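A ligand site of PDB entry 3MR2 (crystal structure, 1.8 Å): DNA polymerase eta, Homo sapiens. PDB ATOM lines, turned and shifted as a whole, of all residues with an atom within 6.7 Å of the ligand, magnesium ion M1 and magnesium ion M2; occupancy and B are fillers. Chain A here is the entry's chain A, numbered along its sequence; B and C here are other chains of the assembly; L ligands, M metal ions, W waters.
OG of Ser 116 is in hydrogen-bond range of N of Asp 118 (2.9 Å).
The backbone carbonyl oxygen (O) of Asp 16 sits at hydrogen-bond distance from the side-chain amino group (NZ) of Lys 234 (3.2 Å).
The backbone NH (N) of Asp 16 is in hydrogen-bond range of the backbone carbonyl oxygen (O) of Ser 216 (2.9 Å).
OG of Ser 116 lies close to N of Glu 119, 3.1 Å away.
The side-chain hydroxyl (OG) of Ser 116 lies close to O3' of DT 9 of chain B, 3.4 Å away.
The guanidinium group (NE) of Arg 58 is in hydrogen-bond range of the backbone carbonyl oxygen (O) of Val 53, at 2.9 Å.
NZ of Lys 234 is in salt-bridge range of OD1 of Asp 18 (2.8 Å).
The side-chain carboxylate of Asp 18 sits at hydrogen-bond distance from the side-chain hydroxyl of Ser 216 (2.8 Å).
OH of Tyr 55 is in hydrogen-bond range of O6 of the ligand, at 2.6 Å.
N3 of the ligand is in hydrogen-bond range of O4 of DT 5 of chain C, 3.0 Å away.
An oxygen (O6) of the ligand lies within hydrogen-bond range of the backbone NH (N) of Cys 19 (2.9 Å).
NH1 of Arg 58 lies within salt-bridge range of O9 of the ligand.
O7 of the ligand lies within hydrogen-bond range of N of Phe 21, 3.0 Å away.
NZ of Lys 234 is in salt-bridge range of O6 of the ligand, 3.1 Å away.
The backbone NH (N) of Phe 20 sits at hydrogen-bond distance from an oxygen (O5) of the ligand (3.3 Å).
Merely in contact with magnesium ion M1: Lys 234 (3.8 Å).
Within 4 Å of magnesium ion M1: Asp 16, Met 17, Asp 118 and Lys 234.
The nearest printed residue that does not touch magnesium ion M1 is Asp 18 (4.3 Å).
Water W8 bridges NE of Arg 64 (2.8 Å) and N3 of the ligand (2.8 Å).
Water W6 lies within hydrogen-bond range of N of Val 53, O5 of the ligand and NH2 of Arg 58.
The guanidinium group (NH2) of Arg 64 lies close to a nitrogen (N3) of the ligand (3.4 Å).
Residues that only touch the ligand: Asp 18 (3.3 Å), Ile 51 (3.4 Å), Ala 52 (3.5 Å), DA 6 of chain C (3.6 Å) and Ile 117 (3.8 Å).
Hydrophobic or aromatic side chains within 4 Å of the ligand: Phe 20, Phe 21, Ala 52, Tyr 55 and Ile 117.
Within 4 Å of the ligand: Asp 16, Met 17, Asp 18, Cys 19, Phe 20, Phe 21, Ile 51, Ala 52, Tyr 55, Arg 58, Arg 64, Ile 117, Asp 118, Lys 234, DT 9 of chain B, DT 5 of chain C and DA 6 of chain C.
Residues that only touch magnesium ion M2: Ser 116 (3.8 Å).
Of the 27 residues printed, 5 come within 4 Å of magnesium ion M2.
The nearest printed residue that does not touch magnesium ion M2 is Met 17 (5.4 Å).
Magnesium ion M1 is bound by OD1 of Asp 118, at 2.1 Å.
Magnesium ion M1 is bound by O of Met 17 (2.1 Å).
OD1 of Asp 16 is bound to magnesium ion M1, at 2.1 Å.
Magnesium ion M1 is bound by O2 of the ligand.
Magnesium ion M1 is bound by an oxygen (O3) of the ligand, 2.2 Å away.
Magnesium ion M1 is bound by O1 of the ligand, at 2.3 Å.
OD2 of Asp 118 binds magnesium ion M2 (2.0 Å).
OD2 of Asp 16 binds magnesium ion M2 (2.0 Å).
OE2 of Glu 119 binds magnesium ion M2, 2.1 Å away.
Water W2 is bound to magnesium ion M2, 2.2 Å away.
Magnesium ion M2 is bound by O3' of DT 9 of chain B, 2.2 Å away.
O1 of the ligand is bound to magnesium ion M2.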
ATOM      1  N   VAL A  15      -0.213 -10.951  28.995  1.00  0.00           N
ATOM      2  CA  VAL A  15       0.671 -11.067  27.834  1.00  0.00           C
ATOM      3  C   VAL A  15       1.754  -9.999  27.901  1.00  0.00           C
ATOM      4  O   VAL A  15       1.400  -8.830  28.132  1.00  0.00           O
ATOM      5  CB  VAL A  15      -0.138 -10.848  26.529  1.00  0.00           C
ATOM      6  CG1 VAL A  15       0.749 -10.982  25.278  1.00  0.00           C
ATOM      7  CG2 VAL A  15      -1.263 -11.886  26.460  1.00  0.00           C
ATOM      8  N   ASP A  16       3.044 -10.422  27.877  1.00  0.00           N
ATOM      9  CA  ASP A  16       4.112  -9.456  27.956  1.00  0.00           C
ATOM     10  C   ASP A  16       5.080  -9.634  26.798  1.00  0.00           C
ATOM     11  O   ASP A  16       5.526 -10.789  26.583  1.00  0.00           O
ATOM     12  CB  ASP A  16       4.847  -9.673  29.287  1.00  0.00           C
ATOM     13  CG  ASP A  16       5.957  -8.665  29.501  1.00  0.00           C
ATOM     14  OD1 ASP A  16       6.999  -8.871  28.886  1.00  0.00           O
ATOM     15  OD2 ASP A  16       5.747  -7.648  30.223  1.00  0.00           O
ATOM     16  N   MET A  17       5.456  -8.564  26.104  1.00  0.00           N
ATOM     17  CA  MET A  17       6.354  -8.686  24.966  1.00  0.00           C
ATOM     18  C   MET A  17       7.768  -9.076  25.403  1.00  0.00           C
ATOM     19  O   MET A  17       8.269  -8.660  26.427  1.00  0.00           O
ATOM     20  CB  MET A  17       6.398  -7.379  24.185  1.00  0.00           C
ATOM     21  CG  MET A  17       5.044  -6.779  23.843  1.00  0.00           C
ATOM     22  SD  MET A  17       3.943  -7.873  22.913  1.00  0.00           S
ATOM     23  CE  MET A  17       4.995  -8.206  21.414  1.00  0.00           C
ATOM     24  N   ASP A  18       8.415  -9.882  24.571  1.00  0.00           N
ATOM     25  CA  ASP A  18       9.802 -10.278  24.880  1.00  0.00           C
ATOM     26  C   ASP A  18      10.775  -9.172  24.469  1.00  0.00           C
ATOM     27  O   ASP A  18      10.565  -8.613  23.364  1.00  0.00           O
ATOM     28  CB  ASP A  18      10.124 -11.558  24.134  1.00  0.00           C
ATOM     29  CG  ASP A  18       9.227 -12.752  24.572  1.00  0.00           C
ATOM     30  OD1 ASP A  18       8.750 -12.836  25.726  1.00  0.00           O
ATOM     31  OD2 ASP A  18       8.982 -13.664  23.739  1.00  0.00           O
ATOM     32  N   CYS A  19      11.741  -8.857  25.349  1.00  0.00           N
ATOM     33  CA  CYS A  19      12.720  -7.770  25.065  1.00  0.00           C
ATOM     34  C   CYS A  19      12.127  -6.750  24.110  1.00  0.00           C
ATOM     35  O   CYS A  19      12.672  -6.464  23.003  1.00  0.00           O
ATOM     36  CB  CYS A  19      14.018  -8.335  24.487  1.00  0.00           C
ATOM     37  SG  CYS A  19      13.954  -9.473  23.031  1.00  0.00           S
ATOM     38  N   PHE A  20      11.058  -6.121  24.558  1.00  0.00           N
ATOM     39  CA  PHE A  20      10.166  -5.356  23.665  1.00  0.00           C
ATOM     40  C   PHE A  20      10.900  -4.257  22.901  1.00  0.00           C
ATOM     41  O   PHE A  20      10.824  -4.219  21.668  1.00  0.00           O
ATOM     42  CB  PHE A  20       9.012  -4.735  24.478  1.00  0.00           C
ATOM     43  CG  PHE A  20       8.039  -4.031  23.618  1.00  0.00           C
ATOM     44  CD1 PHE A  20       7.558  -4.650  22.463  1.00  0.00           C
ATOM     45  CD2 PHE A  20       7.612  -2.789  23.959  1.00  0.00           C
ATOM     46  CE1 PHE A  20       6.615  -3.980  21.644  1.00  0.00           C
ATOM     47  CE2 PHE A  20       6.683  -2.135  23.146  1.00  0.00           C
ATOM     48  CZ  PHE A  20       6.190  -2.761  21.979  1.00  0.00           C
ATOM     49  N   PHE A  21      11.561  -3.282  23.579  1.00  0.00           N
ATOM     50  CA  PHE A  21      12.193  -2.216  22.758  1.00  0.00           C
ATOM     51  C   PHE A  21      13.213  -2.806  21.772  1.00  0.00           C
ATOM     52  O   PHE A  21      13.413  -2.261  20.665  1.00  0.00           O
ATOM     53  CB  PHE A  21      12.867  -1.169  23.645  1.00  0.00           C
ATOM     54  CG  PHE A  21      11.919  -0.283  24.388  1.00  0.00           C
ATOM     55  CD1 PHE A  21      10.603  -0.635  24.556  1.00  0.00           C
ATOM     56  CD2 PHE A  21      12.364   0.906  24.923  1.00  0.00           C
ATOM     57  CE1 PHE A  21       9.707   0.193  25.297  1.00  0.00           C
ATOM     58  CE2 PHE A  21      11.492   1.757  25.655  1.00  0.00           C
ATOM     59  CZ  PHE A  21      10.177   1.394  25.846  1.00  0.00           C
ATOM     60  N   VAL A  22      13.891  -3.862  22.151  1.00  0.00           N
ATOM     61  CA  VAL A  22      14.820  -4.464  21.190  1.00  0.00           C
ATOM     62  C   VAL A  22      14.077  -4.988  19.950  1.00  0.00           C
ATOM     63  O   VAL A  22      14.540  -4.789  18.788  1.00  0.00           O
ATOM     64  CB  VAL A  22      15.584  -5.644  21.850  1.00  0.00           C
ATOM     65  CG1 VAL A  22      16.270  -6.525  20.779  1.00  0.00           C
ATOM     66  CG2 VAL A  22      16.669  -5.052  22.755  1.00  0.00           C
ATOM     67  N   GLN A  41      20.025   4.656  25.920  1.00  0.00           N
ATOM     68  CA  GLN A  41      19.716   6.085  25.815  1.00  0.00           C
ATOM     69  C   GLN A  41      20.891   6.942  26.258  1.00  0.00           C
ATOM     70  O   GLN A  41      21.615   6.534  27.203  1.00  0.00           O
ATOM     71  CB  GLN A  41      18.485   6.445  26.650  1.00  0.00           C
ATOM     72  CG  GLN A  41      18.520   5.984  28.088  1.00  0.00           C
ATOM     73  CD  GLN A  41      17.154   6.124  28.794  1.00  0.00           C
ATOM     74  OE1 GLN A  41      16.064   6.222  28.162  1.00  0.00           O
ATOM     75  NE2 GLN A  41      17.213   6.099  30.114  1.00  0.00           N
ATOM     76  N   ILE A  51      18.408   0.048  28.373  1.00  0.00           N
ATOM     77  CA  ILE A  51      17.043  -0.077  28.871  1.00  0.00           C
ATOM     78  C   ILE A  51      16.370  -1.346  28.386  1.00  0.00           C
ATOM     79  O   ILE A  51      15.356  -1.739  28.977  1.00  0.00           O
ATOM     80  CB  ILE A  51      16.176   1.114  28.549  1.00  0.00           C
ATOM     81  CG1 ILE A  51      16.072   1.305  27.033  1.00  0.00           C
ATOM     82  CG2 ILE A  51      16.785   2.345  29.222  1.00  0.00           C
ATOM     83  CD1 ILE A  51      15.135   2.504  26.687  1.00  0.00           C
ATOM     84  N   ALA A  52      16.934  -2.066  27.412  1.00  0.00           N
ATOM     85  CA  ALA A  52      16.356  -3.343  26.977  1.00  0.00           C
ATOM     86  C   ALA A  52      17.445  -4.263  26.420  1.00  0.00           C
ATOM     87  O   ALA A  52      18.400  -3.735  25.767  1.00  0.00           O
ATOM     88  CB  ALA A  52      15.232  -3.096  25.948  1.00  0.00           C
ATOM     89  N   VAL A  53      17.309  -5.582  26.568  1.00  0.00           N
ATOM     90  CA  VAL A  53      18.382  -6.464  26.187  1.00  0.00           C
ATOM     91  C   VAL A  53      17.862  -7.735  25.536  1.00  0.00           C
ATOM     92  O   VAL A  53      16.989  -8.416  26.082  1.00  0.00           O
ATOM     93  CB  VAL A  53      19.173  -6.973  27.488  1.00  0.00           C
ATOM     94  CG1 VAL A  53      20.429  -7.691  26.985  1.00  0.00           C
ATOM     95  CG2 VAL A  53      19.570  -5.767  28.330  1.00  0.00           C
ATOM     96  N   TYR A  55      17.694 -11.610  24.197  1.00  0.00           N
ATOM     97  CA  TYR A  55      18.017 -12.801  24.980  1.00  0.00           C
ATOM     98  C   TYR A  55      19.398 -13.338  24.620  1.00  0.00           C
ATOM     99  O   TYR A  55      20.091 -13.891  25.477  1.00  0.00           O
ATOM    100  CB  TYR A  55      16.959 -13.866  24.774  1.00  0.00           C
ATOM    101  CG  TYR A  55      15.743 -13.589  25.623  1.00  0.00           C
ATOM    102  CD1 TYR A  55      14.803 -12.643  25.240  1.00  0.00           C
ATOM    103  CD2 TYR A  55      15.569 -14.216  26.880  1.00  0.00           C
ATOM    104  CE1 TYR A  55      13.692 -12.317  26.072  1.00  0.00           C
ATOM    105  CE2 TYR A  55      14.513 -13.893  27.713  1.00  0.00           C
ATOM    106  CZ  TYR A  55      13.581 -12.963  27.312  1.00  0.00           C
ATOM    107  OH  TYR A  55      12.490 -12.669  28.142  1.00  0.00           O
ATOM    108  N   ARG A  58      21.594 -11.393  26.873  1.00  0.00           N
ATOM    109  CA  ARG A  58      21.463 -11.820  28.315  1.00  0.00           C
ATOM    110  C   ARG A  58      22.378 -13.012  28.626  1.00  0.00           C
ATOM    111  O   ARG A  58      22.807 -13.151  29.796  1.00  0.00           O
ATOM    112  CB  ARG A  58      20.008 -12.200  28.626  1.00  0.00           C
ATOM    113  CG  ARG A  58      19.118 -10.987  28.522  1.00  0.00           C
ATOM    114  CD  ARG A  58      17.677 -11.331  28.799  1.00  0.00           C
ATOM    115  NE  ARG A  58      16.777 -10.258  28.262  1.00  0.00           N
ATOM    116  CZ  ARG A  58      15.507 -10.081  28.612  1.00  0.00           C
ATOM    117  NH1 ARG A  58      14.908 -10.883  29.504  1.00  0.00           N
ATOM    118  NH2 ARG A  58      14.778  -9.088  28.056  1.00  0.00           N
ATOM    119  N   ARG A  64      19.662  -4.678  32.079  1.00  0.00           N
ATOM    120  CA  ARG A  64      19.131  -3.336  32.160  1.00  0.00           C
ATOM    121  C   ARG A  64      19.861  -2.494  33.219  1.00  0.00           C
ATOM    122  O   ARG A  64      20.286  -3.036  34.219  1.00  0.00           O
ATOM    123  CB  ARG A  64      17.651  -3.457  32.543  1.00  0.00           C
ATOM    124  CG  ARG A  64      16.969  -2.142  32.865  1.00  0.00           C
ATOM    125  CD  ARG A  64      15.490  -2.345  33.187  1.00  0.00           C
ATOM    126  NE  ARG A  64      15.265  -3.058  34.447  1.00  0.00           N
ATOM    127  CZ  ARG A  64      15.473  -2.541  35.657  1.00  0.00           C
ATOM    128  NH1 ARG A  64      15.227  -3.287  36.722  1.00  0.00           N
ATOM    129  NH2 ARG A  64      15.939  -1.314  35.821  1.00  0.00           N
ATOM    130  N   LEU A  92      10.243   8.499  23.425  1.00  0.00           N
ATOM    131  CA  LEU A  92       9.817   7.050  23.372  1.00  0.00           C
ATOM    132  C   LEU A  92       8.618   6.828  22.424  1.00  0.00           C
ATOM    133  O   LEU A  92       8.034   5.743  22.444  1.00  0.00           O
ATOM    134  CB  LEU A  92       9.457   6.606  24.804  1.00  0.00           C
ATOM    135  CG  LEU A  92      10.593   6.772  25.809  1.00  0.00           C
ATOM    136  CD1 LEU A  92      10.248   6.140  27.158  1.00  0.00           C
ATOM    137  CD2 LEU A  92      11.835   6.112  25.244  1.00  0.00           C
ATOM    138  N   SER A 116       1.322  -1.871  31.212  1.00  0.00           N
ATOM    139  CA  SER A 116       2.610  -1.213  30.944  1.00  0.00           C
ATOM    140  C   SER A 116       2.719  -0.932  29.456  1.00  0.00           C
ATOM    141  O   SER A 116       1.761  -1.254  28.713  1.00  0.00           O
ATOM    142  CB  SER A 116       3.787  -2.088  31.404  1.00  0.00           C
ATOM    143  OG  SER A 116       4.120  -3.132  30.412  1.00  0.00           O
ATOM    144  N   ILE A 117       3.826  -0.341  29.030  1.00  0.00           N
ATOM    145  CA  ILE A 117       3.936  -0.158  27.586  1.00  0.00           C
ATOM    146  C   ILE A 117       4.031  -1.508  26.858  1.00  0.00           C
ATOM    147  O   ILE A 117       3.707  -1.521  25.627  1.00  0.00           O
ATOM    148  CB  ILE A 117       5.257   0.648  27.273  1.00  0.00           C
ATOM    149  CG1 ILE A 117       5.157   1.228  25.858  1.00  0.00           C
ATOM    150  CG2 ILE A 117       6.507  -0.235  27.388  1.00  0.00           C
ATOM    151  CD1 ILE A 117       6.260   2.325  25.586  1.00  0.00           C
ATOM    152  N   ASP A 118       4.429  -2.618  27.532  1.00  0.00           N
ATOM    153  CA  ASP A 118       4.578  -3.863  26.778  1.00  0.00           C
ATOM    154  C   ASP A 118       3.714  -4.999  27.369  1.00  0.00           C
ATOM    155  O   ASP A 118       3.925  -6.186  27.000  1.00  0.00           O
ATOM    156  CB  ASP A 118       6.058  -4.288  26.709  1.00  0.00           C
ATOM    157  CG  ASP A 118       6.438  -5.233  27.839  1.00  0.00           C
ATOM    158  OD1 ASP A 118       7.158  -6.183  27.441  1.00  0.00           O
ATOM    159  OD2 ASP A 118       6.111  -5.008  29.040  1.00  0.00           O
ATOM    160  N   GLU A 119       2.667  -4.736  28.191  1.00  0.00           N
ATOM    161  CA  GLU A 119       1.874  -5.899  28.675  1.00  0.00           C
ATOM    162  C   GLU A 119       0.460  -5.478  29.046  1.00  0.00           C
ATOM    163  O   GLU A 119       0.207  -4.283  29.416  1.00  0.00           O
ATOM    164  CB  GLU A 119       2.553  -6.548  29.903  1.00  0.00           C
ATOM    165  CG  GLU A 119       2.563  -5.608  31.088  1.00  0.00           C
ATOM    166  CD  GLU A 119       3.793  -5.858  31.964  1.00  0.00           C
ATOM    167  OE1 GLU A 119       3.602  -6.622  32.959  1.00  0.00           O
ATOM    168  OE2 GLU A 119       4.870  -5.335  31.664  1.00  0.00           O
ATOM    169  N   SER A 216       5.401 -13.485  25.395  1.00  0.00           N
ATOM    170  CA  SER A 216       5.044 -14.619  26.297  1.00  0.00           C
ATOM    171  C   SER A 216       3.725 -14.334  27.034  1.00  0.00           C
ATOM    172  O   SER A 216       3.259 -13.213  27.045  1.00  0.00           O
ATOM    173  CB  SER A 216       6.176 -14.838  27.304  1.00  0.00           C
ATOM    174  OG  SER A 216       7.367 -15.189  26.512  1.00  0.00           O
ATOM    175  N   LYS A 234       9.593 -17.558  29.682  1.00  0.00           N
ATOM    176  CA  LYS A 234      10.030 -16.622  28.648  1.00  0.00           C
ATOM    177  C   LYS A 234      11.370 -17.052  28.059  1.00  0.00           C
ATOM    178  O   LYS A 234      12.176 -17.576  28.790  1.00  0.00           O
ATOM    179  CB  LYS A 234      10.248 -15.253  29.330  1.00  0.00           C
ATOM    180  CG  LYS A 234       9.382 -14.129  28.792  1.00  0.00           C
ATOM    181  CD  LYS A 234       9.312 -12.944  29.753  1.00  0.00           C
ATOM    182  CE  LYS A 234       8.121 -12.056  29.413  1.00  0.00           C
ATOM    183  NZ  LYS A 234       8.312 -11.331  28.083  1.00  0.00           N
ATOM    184  N   PRO A 235      11.636 -16.812  26.771  1.00  0.00           N
ATOM    185  CA  PRO A 235      10.809 -16.059  25.820  1.00  0.00           C
ATOM    186  C   PRO A 235       9.972 -17.018  24.931  1.00  0.00           C
ATOM    187  O   PRO A 235      10.232 -18.204  24.818  1.00  0.00           O
ATOM    188  CB  PRO A 235      11.859 -15.331  24.973  1.00  0.00           C
ATOM    189  CG  PRO A 235      12.982 -16.398  24.863  1.00  0.00           C
ATOM    190  CD  PRO A 235      13.005 -17.066  26.246  1.00  0.00           C
ATOM    191  P    DT B   9       7.562  -5.058  37.256  1.00  0.00           P
ATOM    192  OP1  DT B   9       7.217  -6.480  36.978  1.00  0.00           O
ATOM    193  OP2  DT B   9       8.907  -4.706  37.771  1.00  0.00           O
ATOM    194  O5'  DT B   9       7.445  -4.201  35.911  1.00  0.00           O
ATOM    195  C5'  DT B   9       6.187  -4.143  35.160  1.00  0.00           C
ATOM    196  C4'  DT B   9       6.466  -3.367  33.882  1.00  0.00           C
ATOM    197  O4'  DT B   9       6.878  -2.018  34.213  1.00  0.00           O
ATOM    198  C3'  DT B   9       7.622  -3.978  33.078  1.00  0.00           C
ATOM    199  O3'  DT B   9       7.196  -4.019  31.667  1.00  0.00           O
ATOM    200  C2'  DT B   9       8.825  -3.034  33.298  1.00  0.00           C
ATOM    201  C1'  DT B   9       8.147  -1.689  33.608  1.00  0.00           C
ATOM    202  N1   DT B   9       8.916  -0.858  34.583  1.00  0.00           N
ATOM    203  C2   DT B   9       9.196   0.473  34.245  1.00  0.00           C
ATOM    204  O2   DT B   9       8.902   0.962  33.165  1.00  0.00           O
ATOM    205  N3   DT B   9       9.890   1.183  35.213  1.00  0.00           N
ATOM    206  C4   DT B   9      10.329   0.667  36.427  1.00  0.00           C
ATOM    207  O4   DT B   9      10.965   1.395  37.207  1.00  0.00           O
ATOM    208  C5   DT B   9      10.013  -0.727  36.706  1.00  0.00           C
ATOM    209  C7   DT B   9      10.478  -1.306  38.016  1.00  0.00           C
ATOM    210  C6   DT B   9       9.327  -1.417  35.788  1.00  0.00           C
ATOM    211  P    DT C   4      24.400   5.428  39.336  1.00  0.00           P
ATOM    212  OP1  DT C   4      24.199   5.817  40.774  1.00  0.00           O
ATOM    213  OP2  DT C   4      25.229   4.232  39.004  1.00  0.00           O
ATOM    214  O5'  DT C   4      23.028   5.100  38.617  1.00  0.00           O
ATOM    215  C5'  DT C   4      23.140   4.561  37.306  1.00  0.00           C
ATOM    216  C4'  DT C   4      21.852   4.700  36.548  1.00  0.00           C
ATOM    217  O4'  DT C   4      21.154   3.448  36.590  1.00  0.00           O
ATOM    218  C3'  DT C   4      20.959   5.682  37.288  1.00  0.00           C
ATOM    219  O3'  DT C   4      19.947   6.172  36.421  1.00  0.00           O
ATOM    220  C2'  DT C   4      20.307   4.790  38.316  1.00  0.00           C
ATOM    221  C1'  DT C   4      20.006   3.614  37.417  1.00  0.00           C
ATOM    222  N1   DT C   4      19.758   2.362  38.079  1.00  0.00           N
ATOM    223  C2   DT C   4      18.753   1.556  37.589  1.00  0.00           C
ATOM    224  O2   DT C   4      18.069   1.867  36.624  1.00  0.00           O
ATOM    225  N3   DT C   4      18.599   0.372  38.270  1.00  0.00           N
ATOM    226  C4   DT C   4      19.348  -0.052  39.356  1.00  0.00           C
ATOM    227  O4   DT C   4      19.107  -1.150  39.865  1.00  0.00           O
ATOM    228  C5   DT C   4      20.376   0.852  39.795  1.00  0.00           C
ATOM    229  C7   DT C   4      21.236   0.468  40.958  1.00  0.00           C
ATOM    230  C6   DT C   4      20.517   2.000  39.148  1.00  0.00           C
ATOM    231  P    DT C   5      19.512   7.705  36.555  1.00  0.00           P
ATOM    232  OP1  DT C   5      20.762   8.498  36.630  1.00  0.00           O
ATOM    233  OP2  DT C   5      18.494   7.749  37.670  1.00  0.00           O
ATOM    234  O5'  DT C   5      18.740   8.047  35.188  1.00  0.00           O
ATOM    235  C5'  DT C   5      19.426   8.118  33.942  1.00  0.00           C
ATOM    236  C4'  DT C   5      18.358   8.138  32.863  1.00  0.00           C
ATOM    237  O4'  DT C   5      17.642   6.872  32.903  1.00  0.00           O
ATOM    238  C3'  DT C   5      17.281   9.201  33.094  1.00  0.00           C
ATOM    239  O3'  DT C   5      16.829   9.641  31.796  1.00  0.00           O
ATOM    240  C2'  DT C   5      16.185   8.446  33.854  1.00  0.00           C
ATOM    241  C1'  DT C   5      16.265   7.073  33.188  1.00  0.00           C
ATOM    242  N1   DT C   5      15.788   5.899  33.960  1.00  0.00           N
ATOM    243  C2   DT C   5      14.935   5.004  33.337  1.00  0.00           C
ATOM    244  O2   DT C   5      14.578   5.154  32.169  1.00  0.00           O
ATOM    245  N3   DT C   5      14.548   3.933  34.112  1.00  0.00           N
ATOM    246  C4   DT C   5      14.956   3.679  35.428  1.00  0.00           C
ATOM    247  O4   DT C   5      14.578   2.658  35.992  1.00  0.00           O
ATOM    248  C5   DT C   5      15.812   4.658  36.009  1.00  0.00           C
ATOM    249  C7   DT C   5      16.247   4.453  37.436  1.00  0.00           C
ATOM    250  C6   DT C   5      16.187   5.692  35.257  1.00  0.00           C
ATOM    251  P    DA C   6      15.638  10.696  31.709  1.00  0.00           P
ATOM    252  OP1  DA C   6      16.024  11.528  30.556  1.00  0.00           O
ATOM    253  OP2  DA C   6      15.384  11.311  33.002  1.00  0.00           O
ATOM    254  O5'  DA C   6      14.367   9.831  31.320  1.00  0.00           O
ATOM    255  C5'  DA C   6      14.275   9.232  29.999  1.00  0.00           C
ATOM    256  C4'  DA C   6      12.915   8.627  29.804  1.00  0.00           C
ATOM    257  O4'  DA C   6      12.685   7.546  30.744  1.00  0.00           O
ATOM    258  C3'  DA C   6      11.814   9.656  30.026  1.00  0.00           C
ATOM    259  O3'  DA C   6      10.765   9.355  29.098  1.00  0.00           O
ATOM    260  C2'  DA C   6      11.326   9.393  31.439  1.00  0.00           C
ATOM    261  C1'  DA C   6      11.495   7.828  31.495  1.00  0.00           C
ATOM    262  N9   DA C   6      11.706   7.269  32.826  1.00  0.00           N
ATOM    263  C8   DA C   6      12.404   7.761  33.877  1.00  0.00           C
ATOM    264  N7   DA C   6      12.435   6.940  34.912  1.00  0.00           N
ATOM    265  C5   DA C   6      11.700   5.846  34.494  1.00  0.00           C
ATOM    266  C6   DA C   6      11.342   4.654  35.117  1.00  0.00           C
ATOM    267  N6   DA C   6      11.667   4.315  36.387  1.00  0.00           N
ATOM    268  N1   DA C   6      10.607   3.778  34.421  1.00  0.00           N
ATOM    269  C2   DA C   6      10.249   4.078  33.170  1.00  0.00           C
ATOM    270  N3   DA C   6      10.493   5.198  32.464  1.00  0.00           N
ATOM    271  C4   DA C   6      11.231   6.052  33.204  1.00  0.00           C
HETATM  272  N1  LIG L   1      13.279   1.973  32.840  1.00  0.00           N
HETATM  273  C1  LIG L   1      13.040   2.404  31.573  1.00  0.00           C
HETATM  274  N2  LIG L   1      12.451   1.560  30.664  1.00  0.00           N
HETATM  275  C2  LIG L   1      12.118   0.320  31.021  1.00  0.00           C
HETATM  276  C3  LIG L   1      12.386  -0.154  32.361  1.00  0.00           C
HETATM  277  C4  LIG L   1      12.987   0.739  33.265  1.00  0.00           C
HETATM  278  N3  LIG L   1      13.229   0.361  34.525  1.00  0.00           N
HETATM  279  N4  LIG L   1      11.957  -1.453  32.410  1.00  0.00           N
HETATM  280  C5  LIG L   1      11.450  -1.765  31.237  1.00  0.00           C
HETATM  281  N5  LIG L   1      11.538  -0.658  30.369  1.00  0.00           N
HETATM  282  P1  LIG L   1       9.819  -5.519  30.424  1.00  0.00           P
HETATM  283  P2  LIG L   1      11.436  -6.660  28.189  1.00  0.00           P
HETATM  284  P3  LIG L   1      11.225  -9.367  28.785  1.00  0.00           P
HETATM  285  C6  LIG L   1      11.077  -0.570  29.015  1.00  0.00           C
HETATM  286  O1  LIG L   1       8.755  -6.196  29.997  1.00  0.00           O
HETATM  287  O2  LIG L   1      10.225  -6.543  27.490  1.00  0.00           O
HETATM  288  O3  LIG L   1       9.930  -8.958  29.159  1.00  0.00           O
HETATM  289  C7  LIG L   1      12.076  -1.292  28.053  1.00  0.00           C
HETATM  290  O4  LIG L   1      10.087  -5.449  31.842  1.00  0.00           O
HETATM  291  O5  LIG L   1      12.321  -5.941  27.620  1.00  0.00           O
HETATM  292  O6  LIG L   1      11.280 -10.382  27.787  1.00  0.00           O
HETATM  293  C8  LIG L   1      11.514  -2.680  27.760  1.00  0.00           C
HETATM  294  O7  LIG L   1      11.803  -3.336  26.612  1.00  0.00           O
HETATM  295  N6  LIG L   1      11.138  -6.069  29.704  1.00  0.00           N
HETATM  296  O8  LIG L   1      12.020  -8.152  28.253  1.00  0.00           O
HETATM  297  O9  LIG L   1      11.905  -9.823  29.913  1.00  0.00           O
HETATM  298  C9  LIG L   1      10.040  -2.378  28.074  1.00  0.00           C
HETATM  299  O10 LIG L   1       9.906  -1.226  28.874  1.00  0.00           O
HETATM  300  C10 LIG L   1       9.356  -3.666  28.617  1.00  0.00           C
HETATM  301  O11 LIG L   1       9.685  -4.068  29.979  1.00  0.00           O
HETATM  302 MG    MG M   1       8.499  -7.583  28.190  1.00  0.00          MG
HETATM  303 MG    MG M   2       6.642  -5.917  30.748  1.00  0.00          MG
HETATM  304  O   HOH W   1      13.099  -8.250  31.770  1.00  0.00           O
HETATM  305  O   HOH W   2       7.459  -6.969  32.448  1.00  0.00           O
HETATM  306  O   HOH W   3      11.680   3.566  28.613  1.00  0.00           O
HETATM  307  O   HOH W   4       8.986  -9.237  31.721  1.00  0.00           O
HETATM  308  O   HOH W   5      10.442  -6.521  34.352  1.00  0.00           O
HETATM  309  O   HOH W   6      15.111  -6.083  28.131  1.00  0.00           O
HETATM  310  O   HOH W   7       7.403  -1.685  30.424  1.00  0.00           O
HETATM  311  O   HOH W   8      12.673  -2.351  35.138  1.00  0.00           O
